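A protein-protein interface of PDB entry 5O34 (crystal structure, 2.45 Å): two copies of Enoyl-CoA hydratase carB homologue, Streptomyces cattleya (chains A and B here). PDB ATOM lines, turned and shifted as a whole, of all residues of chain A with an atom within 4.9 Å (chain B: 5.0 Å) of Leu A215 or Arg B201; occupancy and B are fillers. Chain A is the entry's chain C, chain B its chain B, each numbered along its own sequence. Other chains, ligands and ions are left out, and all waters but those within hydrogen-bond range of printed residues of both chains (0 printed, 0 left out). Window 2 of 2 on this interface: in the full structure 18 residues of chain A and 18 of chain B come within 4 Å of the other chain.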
ATOM      1  N   TYR A 163      10.613  -7.627 -28.923  1.00  0.00           N
ATOM      2  CA  TYR A 163      10.168  -8.352 -27.740  1.00  0.00           C
ATOM      3  C   TYR A 163       8.686  -8.679 -27.839  1.00  0.00           C
ATOM      4  O   TYR A 163       7.839  -7.779 -27.858  1.00  0.00           O
ATOM      5  CB  TYR A 163      10.473  -7.528 -26.479  1.00  0.00           C
ATOM      6  CG  TYR A 163      10.585  -8.321 -25.197  1.00  0.00           C
ATOM      7  CD1 TYR A 163      11.829  -8.598 -24.636  1.00  0.00           C
ATOM      8  CD2 TYR A 163       9.446  -8.712 -24.491  1.00  0.00           C
ATOM      9  CE1 TYR A 163      11.941  -9.280 -23.424  1.00  0.00           C
ATOM     10  CE2 TYR A 163       9.546  -9.386 -23.273  1.00  0.00           C
ATOM     11  CZ  TYR A 163      10.797  -9.670 -22.745  1.00  0.00           C
ATOM     12  OH  TYR A 163      10.913 -10.331 -21.545  1.00  0.00           O
ATOM     13  N   ALA A 211       1.044 -20.504 -25.949  1.00  0.00           N
ATOM     14  CA  ALA A 211       2.020 -19.599 -25.323  1.00  0.00           C
ATOM     15  C   ALA A 211       3.262 -20.275 -24.720  1.00  0.00           C
ATOM     16  O   ALA A 211       4.377 -19.810 -24.970  1.00  0.00           O
ATOM     17  CB  ALA A 211       1.342 -18.727 -24.266  1.00  0.00           C
ATOM     18  N   GLU A 212       3.078 -21.349 -23.930  1.00  0.00           N
ATOM     19  CA  GLU A 212       4.195 -22.012 -23.256  1.00  0.00           C
ATOM     20  C   GLU A 212       5.115 -22.768 -24.223  1.00  0.00           C
ATOM     21  O   GLU A 212       6.333 -22.770 -24.011  1.00  0.00           O
ATOM     22  CB  GLU A 212       3.725 -22.895 -22.084  1.00  0.00           C
ATOM     23  CG  GLU A 212       3.281 -22.098 -20.857  1.00  0.00           C
ATOM     24  CD  GLU A 212       4.349 -21.356 -20.068  1.00  0.00           C
ATOM     25  OE1 GLU A 212       5.523 -21.793 -20.088  1.00  0.00           O
ATOM     26  OE2 GLU A 212       4.003 -20.354 -19.400  1.00  0.00           O
ATOM     27  N   ARG A 213       4.557 -23.345 -25.305  1.00  0.00           N
ATOM     28  CA  ARG A 213       5.372 -23.987 -26.326  1.00  0.00           C
ATOM     29  C   ARG A 213       6.080 -22.884 -27.139  1.00  0.00           C
ATOM     30  O   ARG A 213       7.259 -23.031 -27.466  1.00  0.00           O
ATOM     31  CB  ARG A 213       4.536 -24.891 -27.247  1.00  0.00           C
ATOM     32  CG  ARG A 213       5.420 -25.842 -28.059  1.00  0.00           C
ATOM     33  CD  ARG A 213       4.726 -26.431 -29.270  1.00  0.00           C
ATOM     34  NE  ARG A 213       3.523 -27.160 -28.893  1.00  0.00           N
ATOM     35  CZ  ARG A 213       2.644 -27.666 -29.746  1.00  0.00           C
ATOM     36  NH1 ARG A 213       2.833 -27.545 -31.058  1.00  0.00           N
ATOM     37  NH2 ARG A 213       1.567 -28.296 -29.299  1.00  0.00           N
ATOM     38  N   ALA A 214       5.366 -21.769 -27.420  1.00  0.00           N
ATOM     39  CA  ALA A 214       5.903 -20.618 -28.158  1.00  0.00           C
ATOM     40  C   ALA A 214       7.080 -20.014 -27.397  1.00  0.00           C
ATOM     41  O   ALA A 214       8.106 -19.726 -28.008  1.00  0.00           O
ATOM     42  CB  ALA A 214       4.819 -19.571 -28.388  1.00  0.00           C
ATOM     43  N   LEU A 215       6.956 -19.900 -26.066  1.00  0.00           N
ATOM     44  CA  LEU A 215       7.998 -19.371 -25.188  1.00  0.00           C
ATOM     45  C   LEU A 215       9.265 -20.217 -25.219  1.00  0.00           C
ATOM     46  O   LEU A 215      10.351 -19.675 -25.391  1.00  0.00           O
ATOM     47  CB  LEU A 215       7.477 -19.231 -23.741  1.00  0.00           C
ATOM     48  CG  LEU A 215       8.439 -18.601 -22.726  1.00  0.00           C
ATOM     49  CD1 LEU A 215       8.637 -17.131 -22.992  1.00  0.00           C
ATOM     50  CD2 LEU A 215       7.944 -18.813 -21.320  1.00  0.00           C
ATOM     51  N   ALA A 216       9.114 -21.538 -25.051  1.00  0.00           N
ATOM     52  CA  ALA A 216      10.184 -22.532 -25.069  1.00  0.00           C
ATOM     53  C   ALA A 216      10.921 -22.546 -26.425  1.00  0.00           C
ATOM     54  O   ALA A 216      12.138 -22.708 -26.456  1.00  0.00           O
ATOM     55  CB  ALA A 216       9.596 -23.911 -24.777  1.00  0.00           C
ATOM     56  N   ASP A 217      10.181 -22.356 -27.530  1.00  0.00           N
ATOM     57  CA  ASP A 217      10.712 -22.333 -28.897  1.00  0.00           C
ATOM     58  C   ASP A 217      11.266 -20.969 -29.356  1.00  0.00           C
ATOM     59  O   ASP A 217      11.877 -20.910 -30.418  1.00  0.00           O
ATOM     60  CB  ASP A 217       9.661 -22.864 -29.889  1.00  0.00           C
ATOM     61  CG  ASP A 217       9.333 -24.347 -29.698  1.00  0.00           C
ATOM     62  OD1 ASP A 217      10.111 -25.049 -28.985  1.00  0.00           O
ATOM     63  OD2 ASP A 217       8.336 -24.825 -30.308  1.00  0.00           O
ATOM     64  N   GLY A 218      11.118 -19.916 -28.548  1.00  0.00           N
ATOM     65  CA  GLY A 218      11.623 -18.588 -28.887  1.00  0.00           C
ATOM     66  C   GLY A 218      10.688 -17.720 -29.710  1.00  0.00           C
ATOM     67  O   GLY A 218      11.097 -16.668 -30.214  1.00  0.00           O
ATOM     68  N   LEU A 219       9.423 -18.147 -29.862  1.00  0.00           N
ATOM     69  CA  LEU A 219       8.400 -17.393 -30.586  1.00  0.00           C
ATOM     70  C   LEU A 219       7.843 -16.279 -29.702  1.00  0.00           C
ATOM     71  O   LEU A 219       7.275 -15.313 -30.204  1.00  0.00           O
ATOM     72  CB  LEU A 219       7.286 -18.318 -31.075  1.00  0.00           C
ATOM     73  CG  LEU A 219       7.648 -19.305 -32.174  1.00  0.00           C
ATOM     74  CD1 LEU A 219       6.478 -20.186 -32.483  1.00  0.00           C
ATOM     75  CD2 LEU A 219       8.109 -18.580 -33.434  1.00  0.00           C
ATOM     76  N   LEU A 220       7.992 -16.430 -28.378  1.00  0.00           N
ATOM     77  CA  LEU A 220       7.632 -15.408 -27.399  1.00  0.00           C
ATOM     78  C   LEU A 220       8.847 -15.220 -26.497  1.00  0.00           C
ATOM     79  O   LEU A 220       9.519 -16.190 -26.145  1.00  0.00           O
ATOM     80  CB  LEU A 220       6.414 -15.806 -26.544  1.00  0.00           C
ATOM     81  CG  LEU A 220       5.038 -15.915 -27.219  1.00  0.00           C
ATOM     82  CD1 LEU A 220       4.029 -16.411 -26.216  1.00  0.00           C
ATOM     83  CD2 LEU A 220       4.566 -14.565 -27.829  1.00  0.00           C
ATOM     84  N   HIS A 221       9.129 -13.979 -26.137  1.00  0.00           N
ATOM     85  CA  HIS A 221      10.214 -13.624 -25.234  1.00  0.00           C
ATOM     86  C   HIS A 221       9.834 -13.851 -23.780  1.00  0.00           C
ATOM     87  O   HIS A 221      10.703 -14.158 -22.966  1.00  0.00           O
ATOM     88  CB  HIS A 221      10.569 -12.149 -25.425  1.00  0.00           C
ATOM     89  CG  HIS A 221      11.195 -11.881 -26.751  1.00  0.00           C
ATOM     90  ND1 HIS A 221      10.453 -11.916 -27.922  1.00  0.00           N
ATOM     91  CD2 HIS A 221      12.478 -11.600 -27.052  1.00  0.00           C
ATOM     92  CE1 HIS A 221      11.306 -11.653 -28.894  1.00  0.00           C
ATOM     93  NE2 HIS A 221      12.534 -11.449 -28.418  1.00  0.00           N
ATOM     94  N   GLU A 222       8.541 -13.652 -23.451  1.00  0.00           N
ATOM     95  CA  GLU A 222       7.995 -13.761 -22.099  1.00  0.00           C
ATOM     96  C   GLU A 222       6.481 -13.980 -22.154  1.00  0.00           C
ATOM     97  O   GLU A 222       5.819 -13.516 -23.084  1.00  0.00           O
ATOM     98  CB  GLU A 222       8.294 -12.451 -21.334  1.00  0.00           C
ATOM     99  CG  GLU A 222       8.134 -12.485 -19.818  1.00  0.00           C
ATOM    100  CD  GLU A 222       8.174 -11.123 -19.130  1.00  0.00           C
ATOM    101  OE1 GLU A 222       8.830 -10.194 -19.659  1.00  0.00           O
ATOM    102  OE2 GLU A 222       7.557 -10.988 -18.047  1.00  0.00           O
ATOM    103  N   THR A 223       5.941 -14.660 -21.133  1.00  0.00           N
ATOM    104  CA  THR A 223       4.502 -14.875 -20.948  1.00  0.00           C
ATOM    105  C   THR A 223       4.075 -14.295 -19.607  1.00  0.00           C
ATOM    106  O   THR A 223       4.844 -14.322 -18.647  1.00  0.00           O
ATOM    107  CB  THR A 223       4.067 -16.359 -21.066  1.00  0.00           C
ATOM    108  OG1 THR A 223       4.641 -17.129 -20.014  1.00  0.00           O
ATOM    109  CG2 THR A 223       4.371 -16.975 -22.420  1.00  0.00           C
ATOM    110  N   THR B 197      16.094 -14.409 -30.054  1.00  0.00           N
ATOM    111  CA  THR B 197      15.173 -14.271 -28.918  1.00  0.00           C
ATOM    112  C   THR B 197      15.909 -14.132 -27.590  1.00  0.00           C
ATOM    113  O   THR B 197      15.665 -13.161 -26.872  1.00  0.00           O
ATOM    114  CB  THR B 197      14.141 -15.411 -28.922  1.00  0.00           C
ATOM    115  OG1 THR B 197      13.429 -15.328 -30.157  1.00  0.00           O
ATOM    116  CG2 THR B 197      13.160 -15.321 -27.755  1.00  0.00           C
ATOM    117  N   VAL B 198      16.807 -15.083 -27.280  1.00  0.00           N
ATOM    118  CA  VAL B 198      17.629 -15.063 -26.060  1.00  0.00           C
ATOM    119  C   VAL B 198      18.433 -13.764 -26.001  1.00  0.00           C
ATOM    120  O   VAL B 198      18.459 -13.102 -24.959  1.00  0.00           O
ATOM    121  CB  VAL B 198      18.525 -16.315 -25.942  1.00  0.00           C
ATOM    122  CG1 VAL B 198      19.585 -16.147 -24.853  1.00  0.00           C
ATOM    123  CG2 VAL B 198      17.675 -17.555 -25.685  1.00  0.00           C
ATOM    124  N   MET B 199      18.997 -13.366 -27.157  1.00  0.00           N
ATOM    125  CA  MET B 199      19.751 -12.135 -27.358  1.00  0.00           C
ATOM    126  C   MET B 199      18.903 -10.908 -26.958  1.00  0.00           C
ATOM    127  O   MET B 199      19.386 -10.044 -26.228  1.00  0.00           O
ATOM    128  CB  MET B 199      20.213 -12.059 -28.826  1.00  0.00           C
ATOM    129  CG  MET B 199      21.065 -10.852 -29.152  1.00  0.00           C
ATOM    130  SD  MET B 199      20.098  -9.382 -29.566  1.00  0.00           S
ATOM    131  CE  MET B 199      19.355  -9.884 -31.142  1.00  0.00           C
ATOM    132  N   GLN B 200      17.649 -10.836 -27.450  1.00  0.00           N
ATOM    133  CA  GLN B 200      16.710  -9.750 -27.161  1.00  0.00           C
ATOM    134  C   GLN B 200      16.297  -9.778 -25.695  1.00  0.00           C
ATOM    135  O   GLN B 200      16.245  -8.721 -25.074  1.00  0.00           O
ATOM    136  CB  GLN B 200      15.502  -9.796 -28.103  1.00  0.00           C
ATOM    137  CG  GLN B 200      15.854  -9.467 -29.560  1.00  0.00           C
ATOM    138  CD  GLN B 200      14.926 -10.082 -30.596  1.00  0.00           C
ATOM    139  OE1 GLN B 200      14.347 -11.165 -30.415  1.00  0.00           O
ATOM    140  NE2 GLN B 200      14.828  -9.445 -31.757  1.00  0.00           N
ATOM    141  N   ARG B 201      16.072 -10.976 -25.114  1.00  0.00           N
ATOM    142  CA  ARG B 201      15.736 -11.089 -23.690  1.00  0.00           C
ATOM    143  C   ARG B 201      16.874 -10.471 -22.839  1.00  0.00           C
ATOM    144  O   ARG B 201      16.624  -9.584 -22.011  1.00  0.00           O
ATOM    145  CB  ARG B 201      15.522 -12.555 -23.270  1.00  0.00           C
ATOM    146  CG  ARG B 201      14.196 -13.194 -23.687  1.00  0.00           C
ATOM    147  CD  ARG B 201      14.192 -14.664 -23.307  1.00  0.00           C
ATOM    148  NE  ARG B 201      13.036 -15.372 -23.855  1.00  0.00           N
ATOM    149  CZ  ARG B 201      13.059 -16.605 -24.361  1.00  0.00           C
ATOM    150  NH1 ARG B 201      14.199 -17.291 -24.405  1.00  0.00           N
ATOM    151  NH2 ARG B 201      11.949 -17.153 -24.846  1.00  0.00           N
ATOM    152  N   MET B 202      18.124 -10.908 -23.098  1.00  0.00           N
ATOM    153  CA  MET B 202      19.313 -10.474 -22.373  1.00  0.00           C
ATOM    154  C   MET B 202      19.637  -8.972 -22.495  1.00  0.00           C
ATOM    155  O   MET B 202      19.876  -8.335 -21.475  1.00  0.00           O
ATOM    156  CB  MET B 202      20.528 -11.330 -22.750  1.00  0.00           C
ATOM    157  CG  MET B 202      20.493 -12.691 -22.120  1.00  0.00           C
ATOM    158  SD  MET B 202      22.123 -13.431 -22.124  1.00  0.00           S
ATOM    159  CE  MET B 202      22.748 -12.933 -20.525  1.00  0.00           C
ATOM    160  N   LEU B 203      19.636  -8.418 -23.715  1.00  0.00           N
ATOM    161  CA  LEU B 203      19.936  -7.008 -23.965  1.00  0.00           C
ATOM    162  C   LEU B 203      18.895  -6.052 -23.394  1.00  0.00           C
ATOM    163  O   LEU B 203      19.263  -5.102 -22.705  1.00  0.00           O
ATOM    164  CB  LEU B 203      20.092  -6.716 -25.473  1.00  0.00           C
ATOM    165  CG  LEU B 203      21.289  -7.290 -26.255  1.00  0.00           C
ATOM    166  CD1 LEU B 203      21.733  -6.321 -27.336  1.00  0.00           C
ATOM    167  CD2 LEU B 203      22.443  -7.669 -25.362  1.00  0.00           C
ATOM    168  N   LEU B 204      17.607  -6.290 -23.694  1.00  0.00           N
ATOM    169  CA  LEU B 204      16.516  -5.410 -23.287  1.00  0.00           C
ATOM    170  C   LEU B 204      16.153  -5.476 -21.812  1.00  0.00           C
ATOM    171  O   LEU B 204      15.771  -4.446 -21.265  1.00  0.00           O
ATOM    172  CB  LEU B 204      15.280  -5.632 -24.166  1.00  0.00           C
ATOM    173  CG  LEU B 204      15.531  -5.411 -25.663  1.00  0.00           C
ATOM    174  CD1 LEU B 204      14.327  -5.784 -26.476  1.00  0.00           C
ATOM    175  CD2 LEU B 204      15.950  -3.970 -25.961  1.00  0.00           C
ATOM    176  N   THR B 205      16.278  -6.638 -21.153  1.00  0.00           N
ATOM    177  CA  THR B 205      15.917  -6.724 -19.726  1.00  0.00           C
ATOM    178  C   THR B 205      17.100  -6.452 -18.802  1.00  0.00           C
ATOM    179  O   THR B 205      16.893  -6.047 -17.652  1.00  0.00           O
ATOM    180  CB  THR B 205      15.226  -8.063 -19.367  1.00  0.00           C
ATOM    181  OG1 THR B 205      16.174  -9.141 -19.350  1.00  0.00           O
ATOM    182  CG2 THR B 205      14.022  -8.381 -20.254  1.00  0.00           C
ATOM    183  N   CYS B 206      18.339  -6.727 -19.286  1.00  0.00           N
ATOM    184  CA  CYS B 206      19.597  -6.609 -18.530  1.00  0.00           C
ATOM    185  C   CYS B 206      19.619  -7.503 -17.283  1.00  0.00           C
ATOM    186  O   CYS B 206      20.471  -7.330 -16.411  1.00  0.00           O
ATOM    187  CB  CYS B 206      19.938  -5.156 -18.206  1.00  0.00           C
ATOM    188  SG  CYS B 206      20.363  -4.176 -19.666  1.00  0.00           S
ATOM    189  N   TRP B 209      21.189 -14.335 -15.826  1.00  0.00           N
ATOM    190  CA  TRP B 209      20.860 -15.678 -16.259  1.00  0.00           C
ATOM    191  C   TRP B 209      21.576 -16.664 -15.345  1.00  0.00           C
ATOM    192  O   TRP B 209      22.773 -16.895 -15.521  1.00  0.00           O
ATOM    193  CB  TRP B 209      21.238 -15.904 -17.736  1.00  0.00           C
ATOM    194  CG  TRP B 209      20.078 -15.843 -18.701  1.00  0.00           C
ATOM    195  CD1 TRP B 209      19.594 -16.867 -19.469  1.00  0.00           C
ATOM    196  CD2 TRP B 209      19.312 -14.683 -19.052  1.00  0.00           C
ATOM    197  NE1 TRP B 209      18.557 -16.420 -20.256  1.00  0.00           N
ATOM    198  CE2 TRP B 209      18.363 -15.083 -20.023  1.00  0.00           C
ATOM    199  CE3 TRP B 209      19.327 -13.339 -18.634  1.00  0.00           C
ATOM    200  CZ2 TRP B 209      17.413 -14.202 -20.547  1.00  0.00           C
ATOM    201  CZ3 TRP B 209      18.389 -12.466 -19.161  1.00  0.00           C
ATOM    202  CH2 TRP B 209      17.435 -12.903 -20.095  1.00  0.00           C
ATOM    203  N   ARG B 213      18.964 -21.636 -16.109  1.00  0.00           N
ATOM    204  CA  ARG B 213      18.283 -20.827 -17.119  1.00  0.00           C
ATOM    205  C   ARG B 213      19.206 -20.665 -18.355  1.00  0.00           C
ATOM    206  O   ARG B 213      18.724 -20.692 -19.490  1.00  0.00           O
ATOM    207  CB  ARG B 213      17.894 -19.462 -16.525  1.00  0.00           C
ATOM    208  CG  ARG B 213      16.939 -18.664 -17.407  1.00  0.00           C
ATOM    209  CD  ARG B 213      16.791 -17.235 -16.933  1.00  0.00           C
ATOM    210  NE  ARG B 213      15.904 -16.463 -17.803  1.00  0.00           N
ATOM    211  CZ  ARG B 213      15.646 -15.165 -17.659  1.00  0.00           C
ATOM    212  NH1 ARG B 213      16.212 -14.474 -16.675  1.00  0.00           N
ATOM    213  NH2 ARG B 213      14.827 -14.548 -18.497  1.00  0.00           N
ATOM    214  N   ASP B 217      18.709 -22.124 -22.229  1.00  0.00           N
ATOM    215  CA  ASP B 217      18.777 -21.145 -23.308  1.00  0.00           C
ATOM    216  C   ASP B 217      19.995 -21.339 -24.243  1.00  0.00           C
ATOM    217  O   ASP B 217      20.110 -20.626 -25.233  1.00  0.00           O
ATOM    218  CB  ASP B 217      18.695 -19.706 -22.739  1.00  0.00           C
ATOM    219  CG  ASP B 217      17.279 -19.268 -22.336  1.00  0.00           C
ATOM    220  OD1 ASP B 217      17.099 -18.083 -21.963  1.00  0.00           O
ATOM    221  OD2 ASP B 217      16.348 -20.102 -22.418  1.00  0.00           O
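The side-chain hydroxyl (OG1) of Thr B197 is in hydrogen-bond range of the backbone carbonyl oxygen (O) of Gly A218, 2.7 Å away. O of Leu A215 sits at hydrogen-bond distance from NH2 of Arg B201 (3.0 Å). NE2 of His A221 lies within hydrogen-bond range of OE1 of Gln B200 (2.7 Å). NH2 of Arg B201 sits at hydrogen-bond distance from O of Leu A220 (2.9 Å). The guanidinium group of Arg B201 is in hydrogen-bond range of the backbone carbonyl oxygen of His A221 (2.8 Å).
The backbone NH (N) of Leu A220 sits at hydrogen-bond distance from the backbone carbonyl oxygen (O) of Ala A214 (3.3 Å). NH1 of Arg B201 is in salt-bridge range of OD1 of Asp B217, at 3.9 Å. OH of Tyr A163 sits at hydrogen-bond distance from OE1 of Glu A222, at 2.8 Å. O of Arg B201 lies within hydrogen-bond range of OG1 of Thr B205, at 2.7 Å.
Tyr A163 touches Thr B205. CD2 of His A221 touches O of Thr B197 (3.6 Å).
Printed residues of chain B within 4 Å of Leu A215: Arg B201 (3.0 Å). Arg B201 touches just these residues of chain A: Leu A215 (3.0 Å), Leu A220 (2.9 Å) and His A221 (2.8 Å). Printed residues of chain A within 4 Å of Thr B197: Gly A218 and His A221. Of the printed residues of chain B, Tyr A163 touches Thr B205 (3.9 Å). Printed residues of chain A within 4 Å of Thr B205: Tyr A163. Asp B217 touches none of the printed residues of chain A. Val B198 touches none of the printed residues of chain A. The nearest residue of chain A that does not touch Arg B201 is Tyr A163 (4.2 Å).
Of the 13 printed residues of chain B, 4 touch a printed residue of chain A. Printed residues of chain B that touch a printed residue of chain A: Thr B197, Gln B200, Arg B201 and Thr B205. Among the printed residues, 7 pairs touch across the chains.
Positions printed for both chains: 213 and 217.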
